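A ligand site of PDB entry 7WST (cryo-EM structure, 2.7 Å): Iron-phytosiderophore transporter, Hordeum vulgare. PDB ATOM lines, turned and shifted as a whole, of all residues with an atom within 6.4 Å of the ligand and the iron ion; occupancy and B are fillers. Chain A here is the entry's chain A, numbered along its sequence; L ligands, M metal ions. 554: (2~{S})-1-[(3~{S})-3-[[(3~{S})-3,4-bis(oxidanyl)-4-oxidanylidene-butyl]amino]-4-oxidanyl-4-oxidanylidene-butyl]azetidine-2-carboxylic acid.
The iron ion is bound by an oxygen (O4) of the ligand (2.0 Å), an oxygen (O6) of the ligand (2.0 Å), an oxygen (O1) of the ligand (2.0 Å), an oxygen (O8) of the ligand (2.0 Å), a nitrogen (N2) of the ligand (2.5 Å) and a nitrogen (N1) of the ligand (2.5 Å).
The iron ion has six donor atoms within binding distance.
An oxygen (O5) of the ligand is in hydrogen-bond range of the side-chain hydroxyl (OH) of Tyr 551 (2.8 Å).
O of Gly 76 lies close to N2 of the ligand, at 3.1 Å.
O7 of the ligand is in hydrogen-bond range of N of Ser 136 (3.4 Å).
OG of Ser 136 sits at hydrogen-bond distance from O7 of the ligand.
The side-chain amino group of Lys 482 lies close to an oxygen (O6) of the ligand.
O7 of the ligand lies within hydrogen-bond range of N of Gly 135, 3.4 Å away.
O6 of the ligand lies close to O of Phe 130 (3.3 Å).
Residues that only touch the ligand: Val 78, Gly 133, Phe 134, Tyr 451, Lys 455, Leu 486 and Tyr 547.
Hydrophobic or aromatic side chains within 4 Å of the ligand: Val 78, Phe 130, Tyr 451, Leu 486, Tyr 547 and Tyr 551.
13 residues have an atom within 4 Å of the ligand: Gly 76, Val 78, Phe 130, Gly 133, Phe 134, Gly 135, Ser 136, Tyr 451, Lys 455, Lys 482, Leu 486, Tyr 547 and Tyr 551.
The nearest printed residue that does not touch the ligand is Ala 72 (4.3 Å).
No residue comes within 4 Å of the iron ion.
The nearest printed residue that does not touch the iron ion is Phe 130 (4.1 Å).
The side-chain hydroxyl (OG) of Ser 136 is in hydrogen-bond range of the side-chain amino group (NZ) of Lys 482 (3.3 Å).
The side-chain amide nitrogen (ND2) of Asn 448 is in hydrogen-bond range of the backbone carbonyl oxygen (O) of Leu 486, at 3.5 Å.
The backbone carbonyl oxygen of Gly 133 sits at hydrogen-bond distance from the side-chain hydroxyl of Thr 137 (3.3 Å).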
ATOM      1  N   ALA A  72      18.165  12.044  -6.987  1.00  0.00           N
ATOM      2  CA  ALA A  72      19.250  12.700  -7.710  1.00  0.00           C
ATOM      3  C   ALA A  72      19.470  14.115  -7.214  1.00  0.00           C
ATOM      4  O   ALA A  72      20.613  14.579  -7.116  1.00  0.00           O
ATOM      5  CB  ALA A  72      18.959  12.678  -9.211  1.00  0.00           C
ATOM      6  N   LEU A  73      18.397  14.838  -6.913  1.00  0.00           N
ATOM      7  CA  LEU A  73      18.490  16.235  -6.511  1.00  0.00           C
ATOM      8  C   LEU A  73      18.748  16.421  -5.016  1.00  0.00           C
ATOM      9  O   LEU A  73      18.836  17.571  -4.571  1.00  0.00           O
ATOM     10  CB  LEU A  73      17.219  16.995  -6.907  1.00  0.00           C
ATOM     11  CG  LEU A  73      16.814  16.965  -8.379  1.00  0.00           C
ATOM     12  CD1 LEU A  73      15.393  17.460  -8.554  1.00  0.00           C
ATOM     13  CD2 LEU A  73      17.789  17.769  -9.219  1.00  0.00           C
ATOM     14  N   THR A  75      20.856  13.741  -3.032  1.00  0.00           N
ATOM     15  CA  THR A  75      22.131  13.109  -2.744  1.00  0.00           C
ATOM     16  C   THR A  75      22.940  12.735  -3.982  1.00  0.00           C
ATOM     17  O   THR A  75      24.155  12.599  -3.883  1.00  0.00           O
ATOM     18  CB  THR A  75      21.927  11.839  -1.901  1.00  0.00           C
ATOM     19  OG1 THR A  75      23.193  11.317  -1.492  1.00  0.00           O
ATOM     20  CG2 THR A  75      21.171  10.775  -2.687  1.00  0.00           C
ATOM     21  N   GLY A  76      22.294  12.583  -5.144  1.00  0.00           N
ATOM     22  CA  GLY A  76      22.982  12.188  -6.344  1.00  0.00           C
ATOM     23  C   GLY A  76      23.346  10.731  -6.429  1.00  0.00           C
ATOM     24  O   GLY A  76      23.977  10.317  -7.412  1.00  0.00           O
ATOM     25  N   LEU A  77      22.960   9.929  -5.438  1.00  0.00           N
ATOM     26  CA  LEU A  77      23.285   8.503  -5.407  1.00  0.00           C
ATOM     27  C   LEU A  77      22.079   7.724  -5.911  1.00  0.00           C
ATOM     28  O   LEU A  77      21.317   7.120  -5.145  1.00  0.00           O
ATOM     29  CB  LEU A  77      23.681   8.077  -3.990  1.00  0.00           C
ATOM     30  CG  LEU A  77      25.113   8.392  -3.550  1.00  0.00           C
ATOM     31  CD1 LEU A  77      25.364   7.845  -2.160  1.00  0.00           C
ATOM     32  CD2 LEU A  77      26.123   7.835  -4.536  1.00  0.00           C
ATOM     33  N   VAL A  78      21.896   7.741  -7.222  1.00  0.00           N
ATOM     34  CA  VAL A  78      20.765   7.086  -7.856  1.00  0.00           C
ATOM     35  C   VAL A  78      20.992   5.580  -7.855  1.00  0.00           C
ATOM     36  O   VAL A  78      22.019   5.115  -8.363  1.00  0.00           O
ATOM     37  CB  VAL A  78      20.536   7.619  -9.283  1.00  0.00           C
ATOM     38  CG1 VAL A  78      19.530   6.748 -10.022  1.00  0.00           C
ATOM     39  CG2 VAL A  78      20.070   9.061  -9.239  1.00  0.00           C
ATOM     40  N   PRO A  79      20.087   4.792  -7.284  1.00  0.00           N
ATOM     41  CA  PRO A  79      20.270   3.342  -7.244  1.00  0.00           C
ATOM     42  C   PRO A  79      19.680   2.646  -8.467  1.00  0.00           C
ATOM     43  O   PRO A  79      18.927   3.222  -9.246  1.00  0.00           O
ATOM     44  CB  PRO A  79      19.514   2.946  -5.970  1.00  0.00           C
ATOM     45  CG  PRO A  79      18.391   3.924  -5.917  1.00  0.00           C
ATOM     46  CD  PRO A  79      18.935   5.226  -6.480  1.00  0.00           C
ATOM     47  N   ALA A 129      15.793  10.002 -16.677  1.00  0.00           N
ATOM     48  CA  ALA A 129      15.821  10.880 -15.524  1.00  0.00           C
ATOM     49  C   ALA A 129      17.225  11.032 -14.956  1.00  0.00           C
ATOM     50  O   ALA A 129      17.631  12.134 -14.575  1.00  0.00           O
ATOM     51  CB  ALA A 129      14.859  10.370 -14.453  1.00  0.00           C
ATOM     52  N   PHE A 130      17.988   9.942 -14.889  1.00  0.00           N
ATOM     53  CA  PHE A 130      19.358  10.004 -14.401  1.00  0.00           C
ATOM     54  C   PHE A 130      20.408   9.909 -15.500  1.00  0.00           C
ATOM     55  O   PHE A 130      21.530  10.390 -15.293  1.00  0.00           O
ATOM     56  CB  PHE A 130      19.609   8.918 -13.349  1.00  0.00           C
ATOM     57  CG  PHE A 130      19.696   7.522 -13.895  1.00  0.00           C
ATOM     58  CD1 PHE A 130      18.569   6.729 -13.966  1.00  0.00           C
ATOM     59  CD2 PHE A 130      20.903   7.000 -14.314  1.00  0.00           C
ATOM     60  CE1 PHE A 130      18.638   5.441 -14.456  1.00  0.00           C
ATOM     61  CE2 PHE A 130      20.975   5.716 -14.817  1.00  0.00           C
ATOM     62  CZ  PHE A 130      19.852   4.932 -14.884  1.00  0.00           C
ATOM     63  N   ALA A 131      20.094   9.312 -16.645  1.00  0.00           N
ATOM     64  CA  ALA A 131      21.004   9.315 -17.777  1.00  0.00           C
ATOM     65  C   ALA A 131      21.063  10.666 -18.483  1.00  0.00           C
ATOM     66  O   ALA A 131      22.075  10.958 -19.130  1.00  0.00           O
ATOM     67  CB  ALA A 131      20.623   8.234 -18.794  1.00  0.00           C
ATOM     68  N   GLY A 132      20.035  11.485 -18.353  1.00  0.00           N
ATOM     69  CA  GLY A 132      19.997  12.796 -18.968  1.00  0.00           C
ATOM     70  C   GLY A 132      20.771  13.869 -18.243  1.00  0.00           C
ATOM     71  O   GLY A 132      20.822  15.005 -18.718  1.00  0.00           O
ATOM     72  N   GLY A 133      21.396  13.539 -17.118  1.00  0.00           N
ATOM     73  CA  GLY A 133      22.160  14.499 -16.366  1.00  0.00           C
ATOM     74  C   GLY A 133      21.323  15.592 -15.763  1.00  0.00           C
ATOM     75  O   GLY A 133      21.735  16.759 -15.713  1.00  0.00           O
ATOM     76  N   PHE A 134      20.128  15.235 -15.288  1.00  0.00           N
ATOM     77  CA  PHE A 134      19.224  16.202 -14.686  1.00  0.00           C
ATOM     78  C   PHE A 134      19.725  16.730 -13.352  1.00  0.00           C
ATOM     79  O   PHE A 134      19.453  17.890 -13.008  1.00  0.00           O
ATOM     80  CB  PHE A 134      17.838  15.588 -14.492  1.00  0.00           C
ATOM     81  CG  PHE A 134      17.002  15.588 -15.744  1.00  0.00           C
ATOM     82  CD1 PHE A 134      16.349  16.733 -16.148  1.00  0.00           C
ATOM     83  CD2 PHE A 134      16.879  14.442 -16.506  1.00  0.00           C
ATOM     84  CE1 PHE A 134      15.585  16.731 -17.297  1.00  0.00           C
ATOM     85  CE2 PHE A 134      16.115  14.440 -17.654  1.00  0.00           C
ATOM     86  CZ  PHE A 134      15.469  15.589 -18.047  1.00  0.00           C
ATOM     87  N   GLY A 135      20.443  15.910 -12.592  1.00  0.00           N
ATOM     88  CA  GLY A 135      21.076  16.335 -11.360  1.00  0.00           C
ATOM     89  C   GLY A 135      22.564  16.536 -11.433  1.00  0.00           C
ATOM     90  O   GLY A 135      23.164  16.955 -10.444  1.00  0.00           O
ATOM     91  N   SER A 136      23.201  16.224 -12.571  1.00  0.00           N
ATOM     92  CA  SER A 136      24.644  16.362 -12.671  1.00  0.00           C
ATOM     93  C   SER A 136      25.073  17.412 -13.686  1.00  0.00           C
ATOM     94  O   SER A 136      25.795  18.357 -13.329  1.00  0.00           O
ATOM     95  CB  SER A 136      25.269  15.011 -13.019  1.00  0.00           C
ATOM     96  OG  SER A 136      24.794  14.537 -14.264  1.00  0.00           O
ATOM     97  N   THR A 137      24.640  17.286 -14.944  1.00  0.00           N
ATOM     98  CA  THR A 137      25.175  18.151 -15.988  1.00  0.00           C
ATOM     99  C   THR A 137      24.196  19.264 -16.352  1.00  0.00           C
ATOM    100  O   THR A 137      24.570  20.444 -16.377  1.00  0.00           O
ATOM    101  CB  THR A 137      25.524  17.342 -17.232  1.00  0.00           C
ATOM    102  OG1 THR A 137      24.382  16.621 -17.683  1.00  0.00           O
ATOM    103  CG2 THR A 137      26.653  16.370 -16.941  1.00  0.00           C
ATOM    104  N   ASN A 448      27.832  -0.804 -15.417  1.00  0.00           N
ATOM    105  CA  ASN A 448      27.694   0.234 -16.425  1.00  0.00           C
ATOM    106  C   ASN A 448      28.655   1.372 -16.123  1.00  0.00           C
ATOM    107  O   ASN A 448      28.575   1.995 -15.058  1.00  0.00           O
ATOM    108  CB  ASN A 448      26.260   0.736 -16.477  1.00  0.00           C
ATOM    109  CG  ASN A 448      25.900   1.373 -17.802  1.00  0.00           C
ATOM    110  OD1 ASN A 448      26.695   2.114 -18.387  1.00  0.00           O
ATOM    111  ND2 ASN A 448      24.696   1.099 -18.282  1.00  0.00           N
ATOM    112  N   GLY A 450      28.975   4.081 -18.089  1.00  0.00           N
ATOM    113  CA  GLY A 450      28.627   5.161 -19.000  1.00  0.00           C
ATOM    114  C   GLY A 450      28.839   6.547 -18.408  1.00  0.00           C
ATOM    115  O   GLY A 450      29.193   7.487 -19.118  1.00  0.00           O
ATOM    116  N   TYR A 451      28.611   6.688 -17.104  1.00  0.00           N
ATOM    117  CA  TYR A 451      28.799   8.004 -16.489  1.00  0.00           C
ATOM    118  C   TYR A 451      30.275   8.312 -16.303  1.00  0.00           C
ATOM    119  O   TYR A 451      30.657   9.473 -16.085  1.00  0.00           O
ATOM    120  CB  TYR A 451      28.059   8.067 -15.149  1.00  0.00           C
ATOM    121  CG  TYR A 451      28.765   7.418 -13.991  1.00  0.00           C
ATOM    122  CD1 TYR A 451      28.654   6.061 -13.749  1.00  0.00           C
ATOM    123  CD2 TYR A 451      29.510   8.184 -13.097  1.00  0.00           C
ATOM    124  CE1 TYR A 451      29.303   5.471 -12.678  1.00  0.00           C
ATOM    125  CE2 TYR A 451      30.149   7.608 -12.023  1.00  0.00           C
ATOM    126  CZ  TYR A 451      30.050   6.251 -11.817  1.00  0.00           C
ATOM    127  OH  TYR A 451      30.684   5.680 -10.751  1.00  0.00           O
ATOM    128  N   LYS A 455      32.400  11.828 -17.990  1.00  0.00           N
ATOM    129  CA  LYS A 455      33.413  12.642 -17.309  1.00  0.00           C
ATOM    130  C   LYS A 455      34.636  12.850 -18.192  1.00  0.00           C
ATOM    131  O   LYS A 455      35.196  13.952 -18.241  1.00  0.00           O
ATOM    132  CB  LYS A 455      33.821  11.984 -16.001  1.00  0.00           C
ATOM    133  CG  LYS A 455      32.726  11.913 -14.958  1.00  0.00           C
ATOM    134  CD  LYS A 455      33.224  11.189 -13.727  1.00  0.00           C
ATOM    135  CE  LYS A 455      32.152  11.067 -12.664  1.00  0.00           C
ATOM    136  NZ  LYS A 455      32.647  10.300 -11.488  1.00  0.00           N
ATOM    137  N   LYS A 482      27.500  10.705 -22.634  1.00  0.00           N
ATOM    138  CA  LYS A 482      27.024   9.836 -21.575  1.00  0.00           C
ATOM    139  C   LYS A 482      25.721   9.154 -21.963  1.00  0.00           C
ATOM    140  O   LYS A 482      25.559   7.941 -21.770  1.00  0.00           O
ATOM    141  CB  LYS A 482      26.835  10.621 -20.274  1.00  0.00           C
ATOM    142  CG  LYS A 482      26.389   9.743 -19.118  1.00  0.00           C
ATOM    143  CD  LYS A 482      26.331  10.497 -17.800  1.00  0.00           C
ATOM    144  CE  LYS A 482      25.087  11.361 -17.704  1.00  0.00           C
ATOM    145  NZ  LYS A 482      24.938  11.958 -16.350  1.00  0.00           N
ATOM    146  N   LEU A 486      25.498   5.374 -22.050  1.00  0.00           N
ATOM    147  CA  LEU A 486      24.816   4.779 -20.903  1.00  0.00           C
ATOM    148  C   LEU A 486      23.551   4.047 -21.337  1.00  0.00           C
ATOM    149  O   LEU A 486      23.234   2.969 -20.812  1.00  0.00           O
ATOM    150  CB  LEU A 486      24.504   5.863 -19.869  1.00  0.00           C
ATOM    151  CG  LEU A 486      24.134   5.482 -18.440  1.00  0.00           C
ATOM    152  CD1 LEU A 486      24.585   6.582 -17.498  1.00  0.00           C
ATOM    153  CD2 LEU A 486      22.646   5.279 -18.314  1.00  0.00           C
ATOM    154  N   ASP A 490      22.606  -0.031 -20.655  1.00  0.00           N
ATOM    155  CA  ASP A 490      21.469  -0.338 -19.798  1.00  0.00           C
ATOM    156  C   ASP A 490      20.371  -1.064 -20.557  1.00  0.00           C
ATOM    157  O   ASP A 490      19.590  -1.824 -19.967  1.00  0.00           O
ATOM    158  CB  ASP A 490      20.917   0.940 -19.163  1.00  0.00           C
ATOM    159  CG  ASP A 490      21.608   1.301 -17.861  1.00  0.00           C
ATOM    160  OD1 ASP A 490      22.183   0.398 -17.214  1.00  0.00           O
ATOM    161  OD2 ASP A 490      21.572   2.487 -17.475  1.00  0.00           O
ATOM    162  N   TYR A 547      26.427  16.863  -7.154  1.00  0.00           N
ATOM    163  CA  TYR A 547      27.125  16.554  -8.399  1.00  0.00           C
ATOM    164  C   TYR A 547      26.929  17.623  -9.458  1.00  0.00           C
ATOM    165  O   TYR A 547      27.644  17.617 -10.467  1.00  0.00           O
ATOM    166  CB  TYR A 547      26.684  15.193  -8.919  1.00  0.00           C
ATOM    167  CG  TYR A 547      27.224  14.054  -8.079  1.00  0.00           C
ATOM    168  CD1 TYR A 547      26.529  13.586  -6.976  1.00  0.00           C
ATOM    169  CD2 TYR A 547      28.437  13.466  -8.380  1.00  0.00           C
ATOM    170  CE1 TYR A 547      27.014  12.556  -6.205  1.00  0.00           C
ATOM    171  CE2 TYR A 547      28.943  12.429  -7.613  1.00  0.00           C
ATOM    172  CZ  TYR A 547      28.225  11.977  -6.526  1.00  0.00           C
ATOM    173  OH  TYR A 547      28.721  10.954  -5.757  1.00  0.00           O
ATOM    174  N   TYR A 551      30.350  18.369 -11.258  1.00  0.00           N
ATOM    175  CA  TYR A 551      30.488  18.339 -12.716  1.00  0.00           C
ATOM    176  C   TYR A 551      30.838  19.715 -13.266  1.00  0.00           C
ATOM    177  O   TYR A 551      31.567  19.825 -14.262  1.00  0.00           O
ATOM    178  CB  TYR A 551      29.200  17.823 -13.358  1.00  0.00           C
ATOM    179  CG  TYR A 551      29.133  16.325 -13.503  1.00  0.00           C
ATOM    180  CD1 TYR A 551      28.934  15.510 -12.397  1.00  0.00           C
ATOM    181  CD2 TYR A 551      29.280  15.720 -14.736  1.00  0.00           C
ATOM    182  CE1 TYR A 551      28.872  14.141 -12.526  1.00  0.00           C
ATOM    183  CE2 TYR A 551      29.221  14.356 -14.878  1.00  0.00           C
ATOM    184  CZ  TYR A 551      29.015  13.564 -13.766  1.00  0.00           C
ATOM    185  OH  TYR A 551      28.956  12.199 -13.908  1.00  0.00           O
HETATM  186  C1  554 L   1      24.764   7.199 -13.405  1.00  0.00           C
HETATM  187  O1  554 L   1      24.704   8.402 -13.762  1.00  0.00           O
HETATM  188  C2  554 L   1      24.994   6.850 -12.005  1.00  0.00           C
HETATM  189  C3  554 L   1      23.756   6.557 -11.280  1.00  0.00           C
HETATM  190  C4  554 L   1      24.183   7.499 -10.222  1.00  0.00           C
HETATM  191  C5  554 L   1      26.506   8.016 -10.548  1.00  0.00           C
HETATM  192  C10 554 L   1      23.237  12.476 -10.304  1.00  0.00           C
HETATM  193  C11 554 L   1      22.554  11.634 -11.387  1.00  0.00           C
HETATM  194  C12 554 L   1      22.905  12.172 -12.766  1.00  0.00           C
HETATM  195  C6  554 L   1      26.657   9.154  -9.534  1.00  0.00           C
HETATM  196  C7  554 L   1      26.425  10.539 -10.136  1.00  0.00           C
HETATM  197  C8  554 L   1      27.098  10.642 -11.513  1.00  0.00           C
HETATM  198  C9  554 L   1      24.743  12.216 -10.233  1.00  0.00           C
HETATM  199  N1  554 L   1      25.190   8.048 -11.159  1.00  0.00           N
HETATM  200  N2  554 L   1      25.009  10.794 -10.269  1.00  0.00           N
HETATM  201  O2  554 L   1      24.623   6.285 -14.260  1.00  0.00           O
HETATM  202  O4  554 L   1      26.395  10.616 -12.552  1.00  0.00           O
HETATM  203  O5  554 L   1      28.343  10.750 -11.598  1.00  0.00           O
HETATM  204  O6  554 L   1      23.880  11.691 -13.402  1.00  0.00           O
HETATM  205  O7  554 L   1      22.211  13.085 -13.287  1.00  0.00           O
HETATM  206  O8  554 L   1      23.002  10.306 -11.287  1.00  0.00           O
HETATM  207 FE    FE M   1      24.530  10.004 -12.579  1.00  0.00          FE
